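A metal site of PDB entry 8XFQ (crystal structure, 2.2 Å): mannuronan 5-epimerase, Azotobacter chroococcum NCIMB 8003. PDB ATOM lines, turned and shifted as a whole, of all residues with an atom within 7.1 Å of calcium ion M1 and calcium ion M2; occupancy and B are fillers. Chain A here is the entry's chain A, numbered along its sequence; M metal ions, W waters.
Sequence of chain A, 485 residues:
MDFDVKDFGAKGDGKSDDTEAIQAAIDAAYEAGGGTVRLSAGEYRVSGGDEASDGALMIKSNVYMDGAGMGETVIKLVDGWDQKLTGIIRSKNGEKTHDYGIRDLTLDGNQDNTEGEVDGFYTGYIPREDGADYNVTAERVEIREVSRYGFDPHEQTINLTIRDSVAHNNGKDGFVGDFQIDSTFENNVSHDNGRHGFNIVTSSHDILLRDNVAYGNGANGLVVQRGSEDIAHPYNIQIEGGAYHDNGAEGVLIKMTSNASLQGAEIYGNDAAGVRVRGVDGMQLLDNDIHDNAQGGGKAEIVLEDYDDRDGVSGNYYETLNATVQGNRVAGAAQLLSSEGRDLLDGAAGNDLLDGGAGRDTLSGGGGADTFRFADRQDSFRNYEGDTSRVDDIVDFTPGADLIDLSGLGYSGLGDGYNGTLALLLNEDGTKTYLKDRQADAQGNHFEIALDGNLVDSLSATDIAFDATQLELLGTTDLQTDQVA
The backbone carbonyl oxygen (O) of Asp 379 binds calcium ion M2. Calcium ion M2 is bound by O of Gly 359 (2.4 Å). OD2 of Asp 361 binds calcium ion M2 (2.4 Å). Water W1 is bound to calcium ion M2 (2.5 Å). Calcium ion M2 is bound by O of Gly 357, 2.5 Å away. Calcium ion M2 is bound by OD1 of Asp 392 (2.6 Å). OD2 of Asp 392 binds calcium ion M2, at 2.7 Å. Calcium ion M2 has seven donor atoms within binding distance.
Calcium ion M1 is bound by O of Ala 358, O of Gly 356, O of Gly 341, OD1 of Asp 361, OD2 of Asp 343 and O of Ser 339. Calcium ion M1 has six donor atoms within binding distance. Slightly farther from calcium ion M1 lies the side-chain carboxylate (OD2) of Asp 361 (3.0 Å).
Within 4 Å of calcium ion M2: Gly 357, Ala 358, Gly 359, Asp 361, Asp 379 and Asp 392. Along chain A the residues within 4 Å of calcium ion M2 span positions 357 to 392.
Six residues have an atom within 4 Å of calcium ion M1: Ser 339, Gly 341, Asp 343, Gly 356, Ala 358 and Asp 361. Along chain A the residues within 4 Å of calcium ion M1 span positions 339 to 361. The nearest printed residue that does not touch calcium ion M1 is Gly 357 (4.2 Å).
The side-chain carboxylate of Asp 343 sits at hydrogen-bond distance from the side-chain hydroxyl of Ser 338 (2.6 Å). The backbone NH of Ala 358 sits at hydrogen-bond distance from the side-chain carboxylate of Asp 379 (3.4 Å). The side-chain carboxylate (OD1) of Asp 355 is in hydrogen-bond range of the backbone NH (N) of Gly 357 (2.9 Å). O of Asp 343 is in hydrogen-bond range of N of Thr 362 (3.0 Å). The backbone NH (N) of Asp 392 lies within hydrogen-bond range of the side-chain hydroxyl (OG) of Ser 380, at 2.8 Å. The backbone carbonyl oxygen (O) of Ser 338 sits at hydrogen-bond distance from the backbone NH (N) of Gly 357. The backbone NH (N) of Asn 322 lies within hydrogen-bond range of the side-chain carboxylate (OD1) of Asp 343 (3.4 Å).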
ATOM      1  N   LEU A 321     -18.048   4.468 -25.627  1.00  0.00           N
ATOM      2  CA  LEU A 321     -17.398   4.139 -24.366  1.00  0.00           C
ATOM      3  C   LEU A 321     -16.316   5.179 -24.092  1.00  0.00           C
ATOM      4  O   LEU A 321     -15.781   5.797 -25.018  1.00  0.00           O
ATOM      5  CB  LEU A 321     -16.766   2.749 -24.391  1.00  0.00           C
ATOM      6  CG  LEU A 321     -17.614   1.502 -24.560  1.00  0.00           C
ATOM      7  CD1 LEU A 321     -16.727   0.321 -24.924  1.00  0.00           C
ATOM      8  CD2 LEU A 321     -18.374   1.205 -23.285  1.00  0.00           C
ATOM      9  N   ASN A 322     -15.989   5.342 -22.817  1.00  0.00           N
ATOM     10  CA  ASN A 322     -14.840   6.117 -22.376  1.00  0.00           C
ATOM     11  C   ASN A 322     -14.852   7.513 -22.984  1.00  0.00           C
ATOM     12  O   ASN A 322     -13.924   7.929 -23.691  1.00  0.00           O
ATOM     13  CB  ASN A 322     -13.546   5.368 -22.702  1.00  0.00           C
ATOM     14  CG  ASN A 322     -13.403   4.086 -21.901  1.00  0.00           C
ATOM     15  OD1 ASN A 322     -13.447   4.097 -20.669  1.00  0.00           O
ATOM     16  ND2 ASN A 322     -13.266   2.963 -22.606  1.00  0.00           N
ATOM     17  N   SER A 338     -23.337   7.373 -22.683  1.00  0.00           N
ATOM     18  CA  SER A 338     -22.188   6.483 -22.725  1.00  0.00           C
ATOM     19  C   SER A 338     -22.535   5.210 -21.957  1.00  0.00           C
ATOM     20  O   SER A 338     -23.661   5.027 -21.491  1.00  0.00           O
ATOM     21  CB  SER A 338     -20.931   7.192 -22.201  1.00  0.00           C
ATOM     22  OG  SER A 338     -19.767   6.452 -22.521  1.00  0.00           O
ATOM     23  N   SER A 339     -21.543   4.340 -21.782  1.00  0.00           N
ATOM     24  CA  SER A 339     -21.779   2.999 -21.254  1.00  0.00           C
ATOM     25  C   SER A 339     -20.631   2.650 -20.307  1.00  0.00           C
ATOM     26  O   SER A 339     -19.927   3.538 -19.810  1.00  0.00           O
ATOM     27  CB  SER A 339     -21.940   1.976 -22.391  1.00  0.00           C
ATOM     28  OG  SER A 339     -22.212   0.689 -21.860  1.00  0.00           O
ATOM     29  N   GLU A 340     -20.478   1.349 -20.027  1.00  0.00           N
ATOM     30  CA  GLU A 340     -19.500   0.812 -19.086  1.00  0.00           C
ATOM     31  C   GLU A 340     -18.163   1.541 -19.130  1.00  0.00           C
ATOM     32  O   GLU A 340     -17.647   1.868 -20.204  1.00  0.00           O
ATOM     33  CB  GLU A 340     -19.284  -0.682 -19.379  1.00  0.00           C
ATOM     34  CG  GLU A 340     -18.310  -1.357 -18.428  1.00  0.00           C
ATOM     35  CD  GLU A 340     -18.836  -1.432 -17.015  1.00  0.00           C
ATOM     36  OE1 GLU A 340     -19.687  -2.306 -16.745  1.00  0.00           O
ATOM     37  OE2 GLU A 340     -18.404  -0.603 -16.173  1.00  0.00           O
ATOM     38  N   GLY A 341     -17.605   1.797 -17.951  1.00  0.00           N
ATOM     39  CA  GLY A 341     -16.403   2.586 -17.800  1.00  0.00           C
ATOM     40  C   GLY A 341     -16.713   3.973 -17.256  1.00  0.00           C
ATOM     41  O   GLY A 341     -17.858   4.407 -17.147  1.00  0.00           O
ATOM     42  N   ARG A 342     -15.636   4.685 -16.917  1.00  0.00           N
ATOM     43  CA  ARG A 342     -15.763   6.007 -16.317  1.00  0.00           C
ATOM     44  C   ARG A 342     -15.951   7.054 -17.417  1.00  0.00           C
ATOM     45  O   ARG A 342     -15.116   7.160 -18.317  1.00  0.00           O
ATOM     46  CB  ARG A 342     -14.547   6.327 -15.472  1.00  0.00           C
ATOM     47  CG  ARG A 342     -14.463   7.774 -15.004  1.00  0.00           C
ATOM     48  CD  ARG A 342     -13.956   7.850 -13.568  1.00  0.00           C
ATOM     49  NE  ARG A 342     -13.827   9.224 -13.094  1.00  0.00           N
ATOM     50  CZ  ARG A 342     -14.840   9.964 -12.665  1.00  0.00           C
ATOM     51  NH1 ARG A 342     -16.080   9.492 -12.618  1.00  0.00           N
ATOM     52  NH2 ARG A 342     -14.601  11.208 -12.254  1.00  0.00           N
ATOM     53  N   ASP A 343     -17.045   7.810 -17.346  1.00  0.00           N
ATOM     54  CA  ASP A 343     -17.323   8.876 -18.285  1.00  0.00           C
ATOM     55  C   ASP A 343     -17.407  10.214 -17.567  1.00  0.00           C
ATOM     56  O   ASP A 343     -17.909  10.285 -16.439  1.00  0.00           O
ATOM     57  CB  ASP A 343     -18.625   8.610 -19.048  1.00  0.00           C
ATOM     58  CG  ASP A 343     -18.548   7.386 -19.935  1.00  0.00           C
ATOM     59  OD1 ASP A 343     -17.954   7.473 -21.030  1.00  0.00           O
ATOM     60  OD2 ASP A 343     -19.102   6.326 -19.551  1.00  0.00           O
ATOM     61  N   LEU A 344     -16.908  11.261 -18.217  1.00  0.00           N
ATOM     62  CA  LEU A 344     -17.007  12.633 -17.729  1.00  0.00           C
ATOM     63  C   LEU A 344     -17.789  13.425 -18.774  1.00  0.00           C
ATOM     64  O   LEU A 344     -17.264  13.741 -19.845  1.00  0.00           O
ATOM     65  CB  LEU A 344     -15.621  13.250 -17.513  1.00  0.00           C
ATOM     66  CG  LEU A 344     -14.585  12.379 -16.803  1.00  0.00           C
ATOM     67  CD1 LEU A 344     -13.238  13.074 -16.771  1.00  0.00           C
ATOM     68  CD2 LEU A 344     -15.051  12.032 -15.410  1.00  0.00           C
ATOM     69  N   LEU A 345     -19.039  13.745 -18.459  1.00  0.00           N
ATOM     70  CA  LEU A 345     -19.948  14.351 -19.418  1.00  0.00           C
ATOM     71  C   LEU A 345     -20.450  15.673 -18.857  1.00  0.00           C
ATOM     72  O   LEU A 345     -21.194  15.697 -17.864  1.00  0.00           O
ATOM     73  CB  LEU A 345     -21.111  13.411 -19.749  1.00  0.00           C
ATOM     74  CG  LEU A 345     -20.719  11.966 -20.085  1.00  0.00           C
ATOM     75  CD1 LEU A 345     -21.945  11.042 -20.108  1.00  0.00           C
ATOM     76  CD2 LEU A 345     -19.968  11.898 -21.400  1.00  0.00           C
ATOM     77  N   ASP A 355     -26.416  10.645 -19.520  1.00  0.00           N
ATOM     78  CA  ASP A 355     -26.516   9.278 -19.030  1.00  0.00           C
ATOM     79  C   ASP A 355     -25.160   8.610 -19.264  1.00  0.00           C
ATOM     80  O   ASP A 355     -24.803   8.314 -20.411  1.00  0.00           O
ATOM     81  CB  ASP A 355     -27.625   8.520 -19.742  1.00  0.00           C
ATOM     82  CG  ASP A 355     -27.936   7.178 -19.074  1.00  0.00           C
ATOM     83  OD1 ASP A 355     -27.076   6.664 -18.325  1.00  0.00           O
ATOM     84  OD2 ASP A 355     -29.041   6.642 -19.311  1.00  0.00           O
ATOM     85  N   GLY A 356     -24.427   8.354 -18.188  1.00  0.00           N
ATOM     86  CA  GLY A 356     -23.159   7.675 -18.290  1.00  0.00           C
ATOM     87  C   GLY A 356     -23.233   6.159 -18.309  1.00  0.00           C
ATOM     88  O   GLY A 356     -22.184   5.515 -18.418  1.00  0.00           O
ATOM     89  N   GLY A 357     -24.425   5.572 -18.201  1.00  0.00           N
ATOM     90  CA  GLY A 357     -24.536   4.125 -18.231  1.00  0.00           C
ATOM     91  C   GLY A 357     -23.832   3.474 -17.051  1.00  0.00           C
ATOM     92  O   GLY A 357     -23.753   4.030 -15.951  1.00  0.00           O
ATOM     93  N   ALA A 358     -23.299   2.282 -17.286  1.00  0.00           N
ATOM     94  CA  ALA A 358     -22.557   1.575 -16.251  1.00  0.00           C
ATOM     95  C   ALA A 358     -21.274   2.313 -15.899  1.00  0.00           C
ATOM     96  O   ALA A 358     -20.805   3.189 -16.636  1.00  0.00           O
ATOM     97  CB  ALA A 358     -22.240   0.145 -16.698  1.00  0.00           C
ATOM     98  N   GLY A 359     -20.694   1.959 -14.747  1.00  0.00           N
ATOM     99  CA  GLY A 359     -19.458   2.549 -14.304  1.00  0.00           C
ATOM    100  C   GLY A 359     -19.663   3.851 -13.555  1.00  0.00           C
ATOM    101  O   GLY A 359     -20.739   4.464 -13.568  1.00  0.00           O
ATOM    102  N   ARG A 360     -18.599   4.305 -12.887  1.00  0.00           N
ATOM    103  CA  ARG A 360     -18.642   5.531 -12.102  1.00  0.00           C
ATOM    104  C   ARG A 360     -18.463   6.731 -13.018  1.00  0.00           C
ATOM    105  O   ARG A 360     -17.397   6.911 -13.615  1.00  0.00           O
ATOM    106  CB  ARG A 360     -17.578   5.509 -11.009  1.00  0.00           C
ATOM    107  CG  ARG A 360     -17.670   6.711 -10.070  1.00  0.00           C
ATOM    108  CD  ARG A 360     -16.630   6.655  -8.962  1.00  0.00           C
ATOM    109  NE  ARG A 360     -15.293   6.971  -9.455  1.00  0.00           N
ATOM    110  CZ  ARG A 360     -14.792   8.200  -9.528  1.00  0.00           C
ATOM    111  NH1 ARG A 360     -15.498   9.260  -9.162  1.00  0.00           N
ATOM    112  NH2 ARG A 360     -13.555   8.364  -9.979  1.00  0.00           N
ATOM    113  N   ASP A 361     -19.487   7.559 -13.129  1.00  0.00           N
ATOM    114  CA  ASP A 361     -19.478   8.692 -14.033  1.00  0.00           C
ATOM    115  C   ASP A 361     -19.668   9.999 -13.268  1.00  0.00           C
ATOM    116  O   ASP A 361     -20.322  10.030 -12.217  1.00  0.00           O
ATOM    117  CB  ASP A 361     -20.570   8.560 -15.100  1.00  0.00           C
ATOM    118  CG  ASP A 361     -20.585   7.194 -15.742  1.00  0.00           C
ATOM    119  OD1 ASP A 361     -19.519   6.750 -16.221  1.00  0.00           O
ATOM    120  OD2 ASP A 361     -21.651   6.551 -15.753  1.00  0.00           O
ATOM    121  N   THR A 362     -19.082  11.061 -13.796  1.00  0.00           N
ATOM    122  CA  THR A 362     -19.263  12.408 -13.287  1.00  0.00           C
ATOM    123  C   THR A 362     -20.004  13.212 -14.342  1.00  0.00           C
ATOM    124  O   THR A 362     -19.527  13.355 -15.471  1.00  0.00           O
ATOM    125  CB  THR A 362     -17.920  13.055 -12.950  1.00  0.00           C
ATOM    126  OG1 THR A 362     -17.274  12.309 -11.919  1.00  0.00           O
ATOM    127  CG2 THR A 362     -18.114  14.485 -12.486  1.00  0.00           C
ATOM    128  N   LEU A 363     -21.167  13.744 -13.969  1.00  0.00           N
ATOM    129  CA  LEU A 363     -22.030  14.455 -14.892  1.00  0.00           C
ATOM    130  C   LEU A 363     -22.259  15.885 -14.421  1.00  0.00           C
ATOM    131  O   LEU A 363     -22.308  16.159 -13.217  1.00  0.00           O
ATOM    132  CB  LEU A 363     -23.371  13.735 -15.062  1.00  0.00           C
ATOM    133  CG  LEU A 363     -23.304  12.207 -15.121  1.00  0.00           C
ATOM    134  CD1 LEU A 363     -24.604  11.581 -14.651  1.00  0.00           C
ATOM    135  CD2 LEU A 363     -22.952  11.732 -16.521  1.00  0.00           C
ATOM    136  N   PHE A 374     -30.844   7.861 -15.229  1.00  0.00           N
ATOM    137  CA  PHE A 374     -30.259   6.625 -14.722  1.00  0.00           C
ATOM    138  C   PHE A 374     -31.184   5.495 -15.140  1.00  0.00           C
ATOM    139  O   PHE A 374     -32.286   5.344 -14.593  1.00  0.00           O
ATOM    140  CB  PHE A 374     -30.074   6.706 -13.204  1.00  0.00           C
ATOM    141  CG  PHE A 374     -29.135   7.794 -12.773  1.00  0.00           C
ATOM    142  CD1 PHE A 374     -29.584   9.099 -12.641  1.00  0.00           C
ATOM    143  CD2 PHE A 374     -27.797   7.518 -12.546  1.00  0.00           C
ATOM    144  CE1 PHE A 374     -28.712  10.108 -12.272  1.00  0.00           C
ATOM    145  CE2 PHE A 374     -26.923   8.519 -12.171  1.00  0.00           C
ATOM    146  CZ  PHE A 374     -27.379   9.829 -12.034  1.00  0.00           C
ATOM    147  N   GLN A 378     -28.013  -0.786 -11.578  1.00  0.00           N
ATOM    148  CA  GLN A 378     -26.600  -1.112 -11.470  1.00  0.00           C
ATOM    149  C   GLN A 378     -25.701  -0.096 -12.172  1.00  0.00           C
ATOM    150  O   GLN A 378     -24.488  -0.319 -12.262  1.00  0.00           O
ATOM    151  CB  GLN A 378     -26.332  -2.507 -12.028  1.00  0.00           C
ATOM    152  CG  GLN A 378     -27.104  -3.593 -11.290  1.00  0.00           C
ATOM    153  CD  GLN A 378     -26.670  -3.726  -9.844  1.00  0.00           C
ATOM    154  OE1 GLN A 378     -27.491  -3.657  -8.932  1.00  0.00           O
ATOM    155  NE2 GLN A 378     -25.373  -3.910  -9.634  1.00  0.00           N
ATOM    156  N   ASP A 379     -26.262   1.007 -12.672  1.00  0.00           N
ATOM    157  CA  ASP A 379     -25.455   2.055 -13.298  1.00  0.00           C
ATOM    158  C   ASP A 379     -24.845   3.005 -12.277  1.00  0.00           C
ATOM    159  O   ASP A 379     -23.963   3.788 -12.654  1.00  0.00           O
ATOM    160  CB  ASP A 379     -26.298   2.851 -14.298  1.00  0.00           C
ATOM    161  CG  ASP A 379     -26.689   2.025 -15.509  1.00  0.00           C
ATOM    162  OD1 ASP A 379     -26.047   0.988 -15.758  1.00  0.00           O
ATOM    163  OD2 ASP A 379     -27.639   2.430 -16.219  1.00  0.00           O
ATOM    164  N   SER A 380     -25.295   2.964 -11.029  1.00  0.00           N
ATOM    165  CA  SER A 380     -24.751   3.831  -9.977  1.00  0.00           C
ATOM    166  C   SER A 380     -25.090   3.166  -8.646  1.00  0.00           C
ATOM    167  O   SER A 380     -26.259   3.175  -8.239  1.00  0.00           O
ATOM    168  CB  SER A 380     -25.364   5.228 -10.060  1.00  0.00           C
ATOM    169  OG  SER A 380     -24.699   6.140  -9.212  1.00  0.00           O
ATOM    170  N   PHE A 381     -24.088   2.597  -7.977  1.00  0.00           N
ATOM    171  CA  PHE A 381     -24.379   1.781  -6.813  1.00  0.00           C
ATOM    172  C   PHE A 381     -23.192   1.706  -5.864  1.00  0.00           C
ATOM    173  O   PHE A 381     -22.048   1.982  -6.232  1.00  0.00           O
ATOM    174  CB  PHE A 381     -24.803   0.358  -7.219  1.00  0.00           C
ATOM    175  CG  PHE A 381     -23.691  -0.442  -7.837  1.00  0.00           C
ATOM    176  CD1 PHE A 381     -23.389  -0.307  -9.190  1.00  0.00           C
ATOM    177  CD2 PHE A 381     -22.956  -1.342  -7.081  1.00  0.00           C
ATOM    178  CE1 PHE A 381     -22.375  -1.041  -9.768  1.00  0.00           C
ATOM    179  CE2 PHE A 381     -21.932  -2.087  -7.658  1.00  0.00           C
ATOM    180  CZ  PHE A 381     -21.638  -1.937  -8.995  1.00  0.00           C
ATOM    181  N   ARG A 390     -18.070   3.357  -8.065  1.00  0.00           N
ATOM    182  CA  ARG A 390     -19.216   2.952  -8.880  1.00  0.00           C
ATOM    183  C   ARG A 390     -20.461   3.775  -8.548  1.00  0.00           C
ATOM    184  O   ARG A 390     -21.537   3.491  -9.108  1.00  0.00           O
ATOM    185  CB  ARG A 390     -19.554   1.458  -8.770  1.00  0.00           C
ATOM    186  CG  ARG A 390     -19.293   0.646 -10.026  1.00  0.00           C
ATOM    187  CD  ARG A 390     -17.860   0.810 -10.530  1.00  0.00           C
ATOM    188  NE  ARG A 390     -16.871   0.221  -9.626  1.00  0.00           N
ATOM    189  CZ  ARG A 390     -15.626   0.653  -9.488  1.00  0.00           C
ATOM    190  NH1 ARG A 390     -15.187   1.694 -10.175  1.00  0.00           N
ATOM    191  NH2 ARG A 390     -14.818   0.031  -8.650  1.00  0.00           N
ATOM    192  N   VAL A 391     -20.377   4.779  -7.679  1.00  0.00           N
ATOM    193  CA  VAL A 391     -21.465   5.720  -7.433  1.00  0.00           C
ATOM    194  C   VAL A 391     -21.228   6.958  -8.282  1.00  0.00           C
ATOM    195  O   VAL A 391     -20.169   7.600  -8.187  1.00  0.00           O
ATOM    196  CB  VAL A 391     -21.582   6.084  -5.948  1.00  0.00           C
ATOM    197  CG1 VAL A 391     -22.597   7.209  -5.766  1.00  0.00           C
ATOM    198  CG2 VAL A 391     -21.982   4.879  -5.120  1.00  0.00           C
ATOM    199  N   ASP A 392     -22.210   7.312  -9.104  1.00  0.00           N
ATOM    200  CA  ASP A 392     -22.143   8.513  -9.913  1.00  0.00           C
ATOM    201  C   ASP A 392     -22.231   9.765  -9.025  1.00  0.00           C
ATOM    202  O   ASP A 392     -22.773   9.730  -7.920  1.00  0.00           O
ATOM    203  CB  ASP A 392     -23.288   8.549 -10.922  1.00  0.00           C
ATOM    204  CG  ASP A 392     -23.045   7.642 -12.111  1.00  0.00           C
ATOM    205  OD1 ASP A 392     -22.058   6.878 -12.099  1.00  0.00           O
ATOM    206  OD2 ASP A 392     -23.858   7.693 -13.060  1.00  0.00           O
HETATM  207 CA    CA M   1     -20.034   5.016 -17.769  1.00  0.00          CA
HETATM  208 CA    CA M   2     -22.894   5.411 -14.041  1.00  0.00          CA
HETATM  209  O   HOH W   1     -25.151   6.140 -14.770  1.00  0.00           O
